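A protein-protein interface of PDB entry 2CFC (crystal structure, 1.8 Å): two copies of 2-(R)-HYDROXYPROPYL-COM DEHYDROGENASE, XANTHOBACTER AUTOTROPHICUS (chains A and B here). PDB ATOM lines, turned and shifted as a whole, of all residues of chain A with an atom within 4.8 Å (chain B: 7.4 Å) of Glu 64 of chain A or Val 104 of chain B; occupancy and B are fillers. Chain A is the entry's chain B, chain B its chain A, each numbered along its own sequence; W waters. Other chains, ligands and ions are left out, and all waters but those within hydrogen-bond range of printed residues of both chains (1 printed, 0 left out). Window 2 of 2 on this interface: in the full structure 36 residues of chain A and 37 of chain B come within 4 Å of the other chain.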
ATOM      1  N   ALA A  62      -7.656  21.787 -17.583  1.00  0.00           N
ATOM      2  CA  ALA A  62      -8.996  22.321 -17.785  1.00  0.00           C
ATOM      3  C   ALA A  62      -9.606  21.844 -19.112  1.00  0.00           C
ATOM      4  O   ALA A  62     -10.793  22.065 -19.373  1.00  0.00           O
ATOM      5  CB  ALA A  62      -8.934  23.843 -17.752  1.00  0.00           C
ATOM      6  N   ASP A  63      -8.794  21.173 -19.933  1.00  0.00           N
ATOM      7  CA  ASP A  63      -9.266  20.708 -21.239  1.00  0.00           C
ATOM      8  C   ASP A  63      -9.500  19.199 -21.257  1.00  0.00           C
ATOM      9  O   ASP A  63      -8.579  18.401 -21.060  1.00  0.00           O
ATOM     10  CB  ASP A  63      -8.251  21.092 -22.316  1.00  0.00           C
ATOM     11  CG  ASP A  63      -8.679  20.644 -23.711  1.00  0.00           C
ATOM     12  OD1 ASP A  63      -9.508  21.337 -24.344  1.00  0.00           O
ATOM     13  OD2 ASP A  63      -8.190  19.595 -24.168  1.00  0.00           O
ATOM     14  N   GLU A  64     -10.737  18.805 -21.540  1.00  0.00           N
ATOM     15  CA  GLU A  64     -11.093  17.389 -21.556  1.00  0.00           C
ATOM     16  C   GLU A  64     -10.253  16.524 -22.496  1.00  0.00           C
ATOM     17  O   GLU A  64      -9.837  15.411 -22.141  1.00  0.00           O
ATOM     18  CB  GLU A  64     -12.562  17.232 -21.906  1.00  0.00           C
ATOM     19  CG  GLU A  64     -13.063  15.816 -21.672  1.00  0.00           C
ATOM     20  CD  GLU A  64     -14.473  15.621 -22.173  1.00  0.00           C
ATOM     21  OE1 GLU A  64     -15.055  16.587 -22.720  1.00  0.00           O
ATOM     22  OE2 GLU A  64     -14.989  14.492 -22.020  1.00  0.00           O
ATOM     23  N   GLY A  65     -10.004  17.025 -23.699  1.00  0.00           N
ATOM     24  CA  GLY A  65      -9.204  16.259 -24.631  1.00  0.00           C
ATOM     25  C   GLY A  65      -7.799  16.005 -24.139  1.00  0.00           C
ATOM     26  O   GLY A  65      -7.304  14.856 -24.204  1.00  0.00           O
ATOM     27  N   ASP A  66      -7.150  17.058 -23.652  1.00  0.00           N
ATOM     28  CA  ASP A  66      -5.782  16.960 -23.136  1.00  0.00           C
ATOM     29  C   ASP A  66      -5.706  15.969 -21.995  1.00  0.00           C
ATOM     30  O   ASP A  66      -4.763  15.146 -21.931  1.00  0.00           O
ATOM     31  CB  ASP A  66      -5.281  18.300 -22.592  1.00  0.00           C
ATOM     32  CG  ASP A  66      -4.904  19.293 -23.677  1.00  0.00           C
ATOM     33  OD1 ASP A  66      -5.056  19.004 -24.876  1.00  0.00           O
ATOM     34  OD2 ASP A  66      -4.430  20.381 -23.305  1.00  0.00           O
ATOM     35  N   VAL A  67      -6.673  16.050 -21.078  1.00  0.00           N
ATOM     36  CA  VAL A  67      -6.683  15.125 -19.946  1.00  0.00           C
ATOM     37  C   VAL A  67      -6.933  13.672 -20.397  1.00  0.00           C
ATOM     38  O   VAL A  67      -6.221  12.729 -19.985  1.00  0.00           O
ATOM     39  CB  VAL A  67      -7.755  15.548 -18.911  1.00  0.00           C
ATOM     40  CG1 VAL A  67      -7.776  14.528 -17.765  1.00  0.00           C
ATOM     41  CG2 VAL A  67      -7.438  16.967 -18.380  1.00  0.00           C
ATOM     42  N   ASN A  68      -7.926  13.470 -21.253  1.00  0.00           N
ATOM     43  CA  ASN A  68      -8.198  12.117 -21.702  1.00  0.00           C
ATOM     44  C   ASN A  68      -7.002  11.494 -22.410  1.00  0.00           C
ATOM     45  O   ASN A  68      -6.692  10.330 -22.183  1.00  0.00           O
ATOM     46  CB  ASN A  68      -9.438  12.084 -22.589  1.00  0.00           C
ATOM     47  CG  ASN A  68     -10.706  12.251 -21.785  1.00  0.00           C
ATOM     48  OD1 ASN A  68     -10.666  12.158 -20.572  1.00  0.00           O
ATOM     49  ND2 ASN A  68     -11.834  12.507 -22.457  1.00  0.00           N
ATOM     50  N   ARG A 116     -12.620  22.374 -12.448  1.00  0.00           N
ATOM     51  CA  ARG A 116     -12.928  21.544 -13.619  1.00  0.00           C
ATOM     52  C   ARG A 116     -11.777  20.588 -13.951  1.00  0.00           C
ATOM     53  O   ARG A 116     -11.994  19.424 -14.351  1.00  0.00           O
ATOM     54  CB  ARG A 116     -13.214  22.425 -14.836  1.00  0.00           C
ATOM     55  CG  ARG A 116     -13.716  21.627 -16.031  1.00  0.00           C
ATOM     56  CD  ARG A 116     -13.957  22.533 -17.256  1.00  0.00           C
ATOM     57  NE  ARG A 116     -14.973  21.981 -18.147  1.00  0.00           N
ATOM     58  CZ  ARG A 116     -14.727  21.554 -19.384  1.00  0.00           C
ATOM     59  NH1 ARG A 116     -13.484  21.603 -19.865  1.00  0.00           N
ATOM     60  NH2 ARG A 116     -15.729  21.140 -20.169  1.00  0.00           N
ATOM     61  N   PHE A 119     -12.050  17.666 -11.688  1.00  0.00           N
ATOM     62  CA  PHE A 119     -13.188  16.815 -12.092  1.00  0.00           C
ATOM     63  C   PHE A 119     -12.776  15.970 -13.302  1.00  0.00           C
ATOM     64  O   PHE A 119     -12.998  14.743 -13.325  1.00  0.00           O
ATOM     65  CB  PHE A 119     -14.389  17.694 -12.486  1.00  0.00           C
ATOM     66  CG  PHE A 119     -15.477  16.957 -13.229  1.00  0.00           C
ATOM     67  CD1 PHE A 119     -16.363  16.117 -12.549  1.00  0.00           C
ATOM     68  CD2 PHE A 119     -15.618  17.118 -14.612  1.00  0.00           C
ATOM     69  CE1 PHE A 119     -17.387  15.444 -13.263  1.00  0.00           C
ATOM     70  CE2 PHE A 119     -16.625  16.455 -15.324  1.00  0.00           C
ATOM     71  CZ  PHE A 119     -17.511  15.618 -14.638  1.00  0.00           C
ATOM     72  N   LEU A 120     -12.146  16.616 -14.279  1.00  0.00           N
ATOM     73  CA  LEU A 120     -11.710  15.930 -15.496  1.00  0.00           C
ATOM     74  C   LEU A 120     -10.652  14.852 -15.205  1.00  0.00           C
ATOM     75  O   LEU A 120     -10.727  13.740 -15.764  1.00  0.00           O
ATOM     76  CB  LEU A 120     -11.191  16.946 -16.505  1.00  0.00           C
ATOM     77  CG  LEU A 120     -12.252  17.897 -17.094  1.00  0.00           C
ATOM     78  CD1 LEU A 120     -11.570  18.938 -18.001  1.00  0.00           C
ATOM     79  CD2 LEU A 120     -13.284  17.103 -17.908  1.00  0.00           C
ATOM     80  N   ARG A 123     -12.451  12.070 -13.410  1.00  0.00           N
ATOM     81  CA  ARG A 123     -13.384  11.413 -14.322  1.00  0.00           C
ATOM     82  C   ARG A 123     -12.606  10.476 -15.241  1.00  0.00           C
ATOM     83  O   ARG A 123     -13.099   9.403 -15.614  1.00  0.00           O
ATOM     84  CB  ARG A 123     -14.145  12.445 -15.182  1.00  0.00           C
ATOM     85  CG  ARG A 123     -15.113  11.828 -16.237  1.00  0.00           C
ATOM     86  CD  ARG A 123     -15.848  12.906 -17.064  1.00  0.00           C
ATOM     87  NE  ARG A 123     -16.675  12.366 -18.159  1.00  0.00           N
ATOM     88  CZ  ARG A 123     -17.847  11.763 -17.976  1.00  0.00           C
ATOM     89  NH1 ARG A 123     -18.323  11.622 -16.751  1.00  0.00           N
ATOM     90  NH2 ARG A 123     -18.553  11.306 -19.004  1.00  0.00           N
ATOM     91  N   LEU B  99     -19.304  11.047  -9.674  1.00  0.00           N
ATOM     92  CA  LEU B  99     -18.396  11.796 -10.522  1.00  0.00           C
ATOM     93  C   LEU B  99     -18.044  11.252 -11.911  1.00  0.00           C
ATOM     94  O   LEU B  99     -18.270  11.938 -12.921  1.00  0.00           O
ATOM     95  CB  LEU B  99     -17.093  12.079  -9.766  1.00  0.00           C
ATOM     96  CG  LEU B  99     -16.233  13.198 -10.375  1.00  0.00           C
ATOM     97  CD1 LEU B  99     -15.303  13.749  -9.280  1.00  0.00           C
ATOM     98  CD2 LEU B  99     -15.454  12.708 -11.603  1.00  0.00           C
ATOM     99  N   THR B 101     -19.343   9.181 -14.018  1.00  0.00           N
ATOM    100  CA  THR B 101     -20.340   9.043 -15.075  1.00  0.00           C
ATOM    101  C   THR B 101     -21.148  10.304 -15.270  1.00  0.00           C
ATOM    102  O   THR B 101     -22.130  10.299 -16.028  1.00  0.00           O
ATOM    103  CB  THR B 101     -21.333   7.921 -14.810  1.00  0.00           C
ATOM    104  OG1 THR B 101     -21.895   8.089 -13.505  1.00  0.00           O
ATOM    105  CG2 THR B 101     -20.646   6.565 -14.914  1.00  0.00           C
ATOM    106  N   THR B 102     -20.806  11.396 -14.587  1.00  0.00           N
ATOM    107  CA  THR B 102     -21.593  12.585 -14.868  1.00  0.00           C
ATOM    108  C   THR B 102     -21.035  13.223 -16.114  1.00  0.00           C
ATOM    109  O   THR B 102     -19.814  13.398 -16.259  1.00  0.00           O
ATOM    110  CB  THR B 102     -21.716  13.624 -13.667  1.00  0.00           C
ATOM    111  OG1 THR B 102     -21.415  14.962 -14.123  1.00  0.00           O
ATOM    112  CG2 THR B 102     -20.935  13.239 -12.506  1.00  0.00           C
ATOM    113  N   PRO B 103     -21.925  13.520 -17.082  1.00  0.00           N
ATOM    114  CA  PRO B 103     -21.581  14.145 -18.369  1.00  0.00           C
ATOM    115  C   PRO B 103     -20.825  15.446 -18.130  1.00  0.00           C
ATOM    116  O   PRO B 103     -21.209  16.239 -17.274  1.00  0.00           O
ATOM    117  CB  PRO B 103     -22.948  14.393 -19.017  1.00  0.00           C
ATOM    118  CG  PRO B 103     -23.813  13.290 -18.436  1.00  0.00           C
ATOM    119  CD  PRO B 103     -23.376  13.253 -16.980  1.00  0.00           C
ATOM    120  N   VAL B 104     -19.755  15.684 -18.874  1.00  0.00           N
ATOM    121  CA  VAL B 104     -19.012  16.922 -18.679  1.00  0.00           C
ATOM    122  C   VAL B 104     -19.957  18.135 -18.794  1.00  0.00           C
ATOM    123  O   VAL B 104     -19.838  19.108 -18.041  1.00  0.00           O
ATOM    124  CB  VAL B 104     -17.877  17.030 -19.712  1.00  0.00           C
ATOM    125  CG1 VAL B 104     -17.199  18.375 -19.598  1.00  0.00           C
ATOM    126  CG2 VAL B 104     -16.862  15.900 -19.483  1.00  0.00           C
ATOM    127  N   GLU B 105     -20.919  18.077 -19.711  1.00  0.00           N
ATOM    128  CA  GLU B 105     -21.844  19.200 -19.877  1.00  0.00           C
ATOM    129  C   GLU B 105     -22.693  19.455 -18.618  1.00  0.00           C
ATOM    130  O   GLU B 105     -23.070  20.604 -18.333  1.00  0.00           O
ATOM    131  CB  GLU B 105     -22.779  18.971 -21.072  1.00  0.00           C
ATOM    132  CG  GLU B 105     -23.772  20.104 -21.260  1.00  0.00           C
ATOM    133  CD  GLU B 105     -25.216  19.718 -20.925  1.00  0.00           C
ATOM    134  OE1 GLU B 105     -25.446  19.059 -19.887  1.00  0.00           O
ATOM    135  OE2 GLU B 105     -26.124  20.081 -21.704  1.00  0.00           O
ATOM    136  N   GLN B 106     -23.002  18.400 -17.874  1.00  0.00           N
ATOM    137  CA  GLN B 106     -23.803  18.560 -16.659  1.00  0.00           C
ATOM    138  C   GLN B 106     -22.964  19.145 -15.544  1.00  0.00           C
ATOM    139  O   GLN B 106     -23.440  19.968 -14.785  1.00  0.00           O
ATOM    140  CB  GLN B 106     -24.405  17.228 -16.214  1.00  0.00           C
ATOM    141  CG  GLN B 106     -25.626  16.800 -17.056  1.00  0.00           C
ATOM    142  CD  GLN B 106     -26.778  17.804 -16.992  1.00  0.00           C
ATOM    143  OE1 GLN B 106     -27.334  18.068 -15.925  1.00  0.00           O
ATOM    144  NE2 GLN B 106     -27.137  18.361 -18.142  1.00  0.00           N
ATOM    145  N   PHE B 107     -21.719  18.695 -15.405  1.00  0.00           N
ATOM    146  CA  PHE B 107     -20.858  19.282 -14.380  1.00  0.00           C
ATOM    147  C   PHE B 107     -20.744  20.802 -14.620  1.00  0.00           C
ATOM    148  O   PHE B 107     -20.834  21.621 -13.686  1.00  0.00           O
ATOM    149  CB  PHE B 107     -19.456  18.705 -14.480  1.00  0.00           C
ATOM    150  CG  PHE B 107     -18.478  19.338 -13.529  1.00  0.00           C
ATOM    151  CD1 PHE B 107     -18.451  18.958 -12.199  1.00  0.00           C
ATOM    152  CD2 PHE B 107     -17.597  20.326 -13.970  1.00  0.00           C
ATOM    153  CE1 PHE B 107     -17.558  19.546 -11.300  1.00  0.00           C
ATOM    154  CE2 PHE B 107     -16.702  20.925 -13.084  1.00  0.00           C
ATOM    155  CZ  PHE B 107     -16.687  20.526 -11.746  1.00  0.00           C
ATOM    156  N   ASP B 108     -20.463  21.166 -15.870  1.00  0.00           N
ATOM    157  CA  ASP B 108     -20.311  22.573 -16.227  1.00  0.00           C
ATOM    158  C   ASP B 108     -21.576  23.359 -15.948  1.00  0.00           C
ATOM    159  O   ASP B 108     -21.498  24.482 -15.427  1.00  0.00           O
ATOM    160  CB  ASP B 108     -19.958  22.733 -17.703  1.00  0.00           C
ATOM    161  CG  ASP B 108     -18.528  22.313 -18.016  1.00  0.00           C
ATOM    162  OD1 ASP B 108     -17.708  22.203 -17.070  1.00  0.00           O
ATOM    163  OD2 ASP B 108     -18.235  22.100 -19.214  1.00  0.00           O
ATOM    164  N   LYS B 109     -22.735  22.796 -16.311  1.00  0.00           N
ATOM    165  CA  LYS B 109     -24.008  23.489 -16.077  1.00  0.00           C
ATOM    166  C   LYS B 109     -24.263  23.714 -14.591  1.00  0.00           C
ATOM    167  O   LYS B 109     -24.628  24.819 -14.163  1.00  0.00           O
ATOM    168  CB  LYS B 109     -25.176  22.702 -16.711  1.00  0.00           C
ATOM    169  CG  LYS B 109     -26.554  23.335 -16.537  1.00  0.00           C
ATOM    170  CD  LYS B 109     -27.645  22.535 -17.271  1.00  0.00           C
ATOM    171  CE  LYS B 109     -28.997  23.258 -17.273  1.00  0.00           C
ATOM    172  NZ  LYS B 109     -29.550  23.427 -15.892  1.00  0.00           N
ATOM    173  N   VAL B 110     -24.073  22.677 -13.778  1.00  0.00           N
ATOM    174  CA  VAL B 110     -24.281  22.802 -12.343  1.00  0.00           C
ATOM    175  C   VAL B 110     -23.325  23.857 -11.764  1.00  0.00           C
ATOM    176  O   VAL B 110     -23.746  24.698 -10.971  1.00  0.00           O
ATOM    177  CB  VAL B 110     -24.098  21.433 -11.634  1.00  0.00           C
ATOM    178  CG1 VAL B 110     -24.117  21.605 -10.099  1.00  0.00           C
ATOM    179  CG2 VAL B 110     -25.255  20.492 -12.049  1.00  0.00           C
HETATM  180  O   HOH W   1     -19.442  13.835 -21.005  1.00  0.00           O
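The side-chain carboxylate (OD2) of Asp 108 of chain B lies within salt-bridge range of the guanidinium group (NH2) of Arg 116 of chain A. The guanidinium group (NH1) of Arg 123 of chain A lies close to the backbone carbonyl oxygen (O) of Thr 102 of chain B, 2.4 Å away.
O of Ala 62 of chain A sits at hydrogen-bond distance from NH1 of Arg 116 of chain A (2.8 Å).
OE2 of Glu 64 of chain A touches CG2 of Val 104 of chain B, at 3.5 Å. NH2 of Arg 116 of chain A touches CG1 of Val 104 of chain B (3.2 Å). CE2 of Phe 107 of chain B touches CA of Arg 116 of chain A (3.9 Å). Phe 119 of chain A touches Leu 99 of chain B (O to CD2, 3.6 Å). Thr 102 of chain B touches Phe 119 of chain A. Phe 119 of chain A touches Phe 107 of chain B. Leu 99 of chain B touches Arg 123 of chain A. Thr 101 of chain B touches Arg 123 of chain A. NE of Arg 123 of chain A touches CG2 of Val 104 of chain B, at 3.8 Å.
Printed residues of chain B within 4 Å of Glu 64 of chain A: Val 104 (3.5 Å). Of the printed residues of chain A, Val 104 of chain B touches Glu 64, Arg 116 and Arg 123. No residue of chain B comes within 4 Å of Gly 65 of chain A. Printed residues of chain A within 4 Å of Thr 102 of chain B: Phe 119 (3.6 Å) and Arg 123 (2.4 Å). Printed residues of chain A within 4 Å of Thr 101 of chain B: Arg 123. Printed residues of chain B within 4 Å of Arg 123 of chain A: Leu 99 (3.6 Å), Thr 101 (3.5 Å), Thr 102 (2.4 Å) and Val 104 (3.8 Å). Of the printed residues of chain B, Arg 116 of chain A touches Val 104, Phe 107 and Asp 108. Printed residues of chain A within 4 Å of Asp 108 of chain B: Arg 116. The nearest printed residue of chain A that does not touch Phe 107 of chain B is Leu 120 of chain A (6.4 Å).
Of the 11 printed residues of chain B, 6 touch a printed residue of chain A. Printed residues of chain B that touch a printed residue of chain A: Leu 99, Thr 101, Thr 102, Val 104, Phe 107 and Asp 108. Hydrophobic or aromatic side chains of chain A within 4 Å of the printed part of chain B: Phe 119. Along chain A the printed residues that touch a printed residue of chain B span positions 64 to 123. Among the printed residues, 11 pairs touch across the chains.
No position is printed for both chains. Of the 11 pairs that touch across the chains among the printed residues, none has its exchanged pair printed and touching as well.
Water W1 lies within hydrogen-bond range of N of Val 104 of chain B and NH2 of Arg 123 of chain A.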
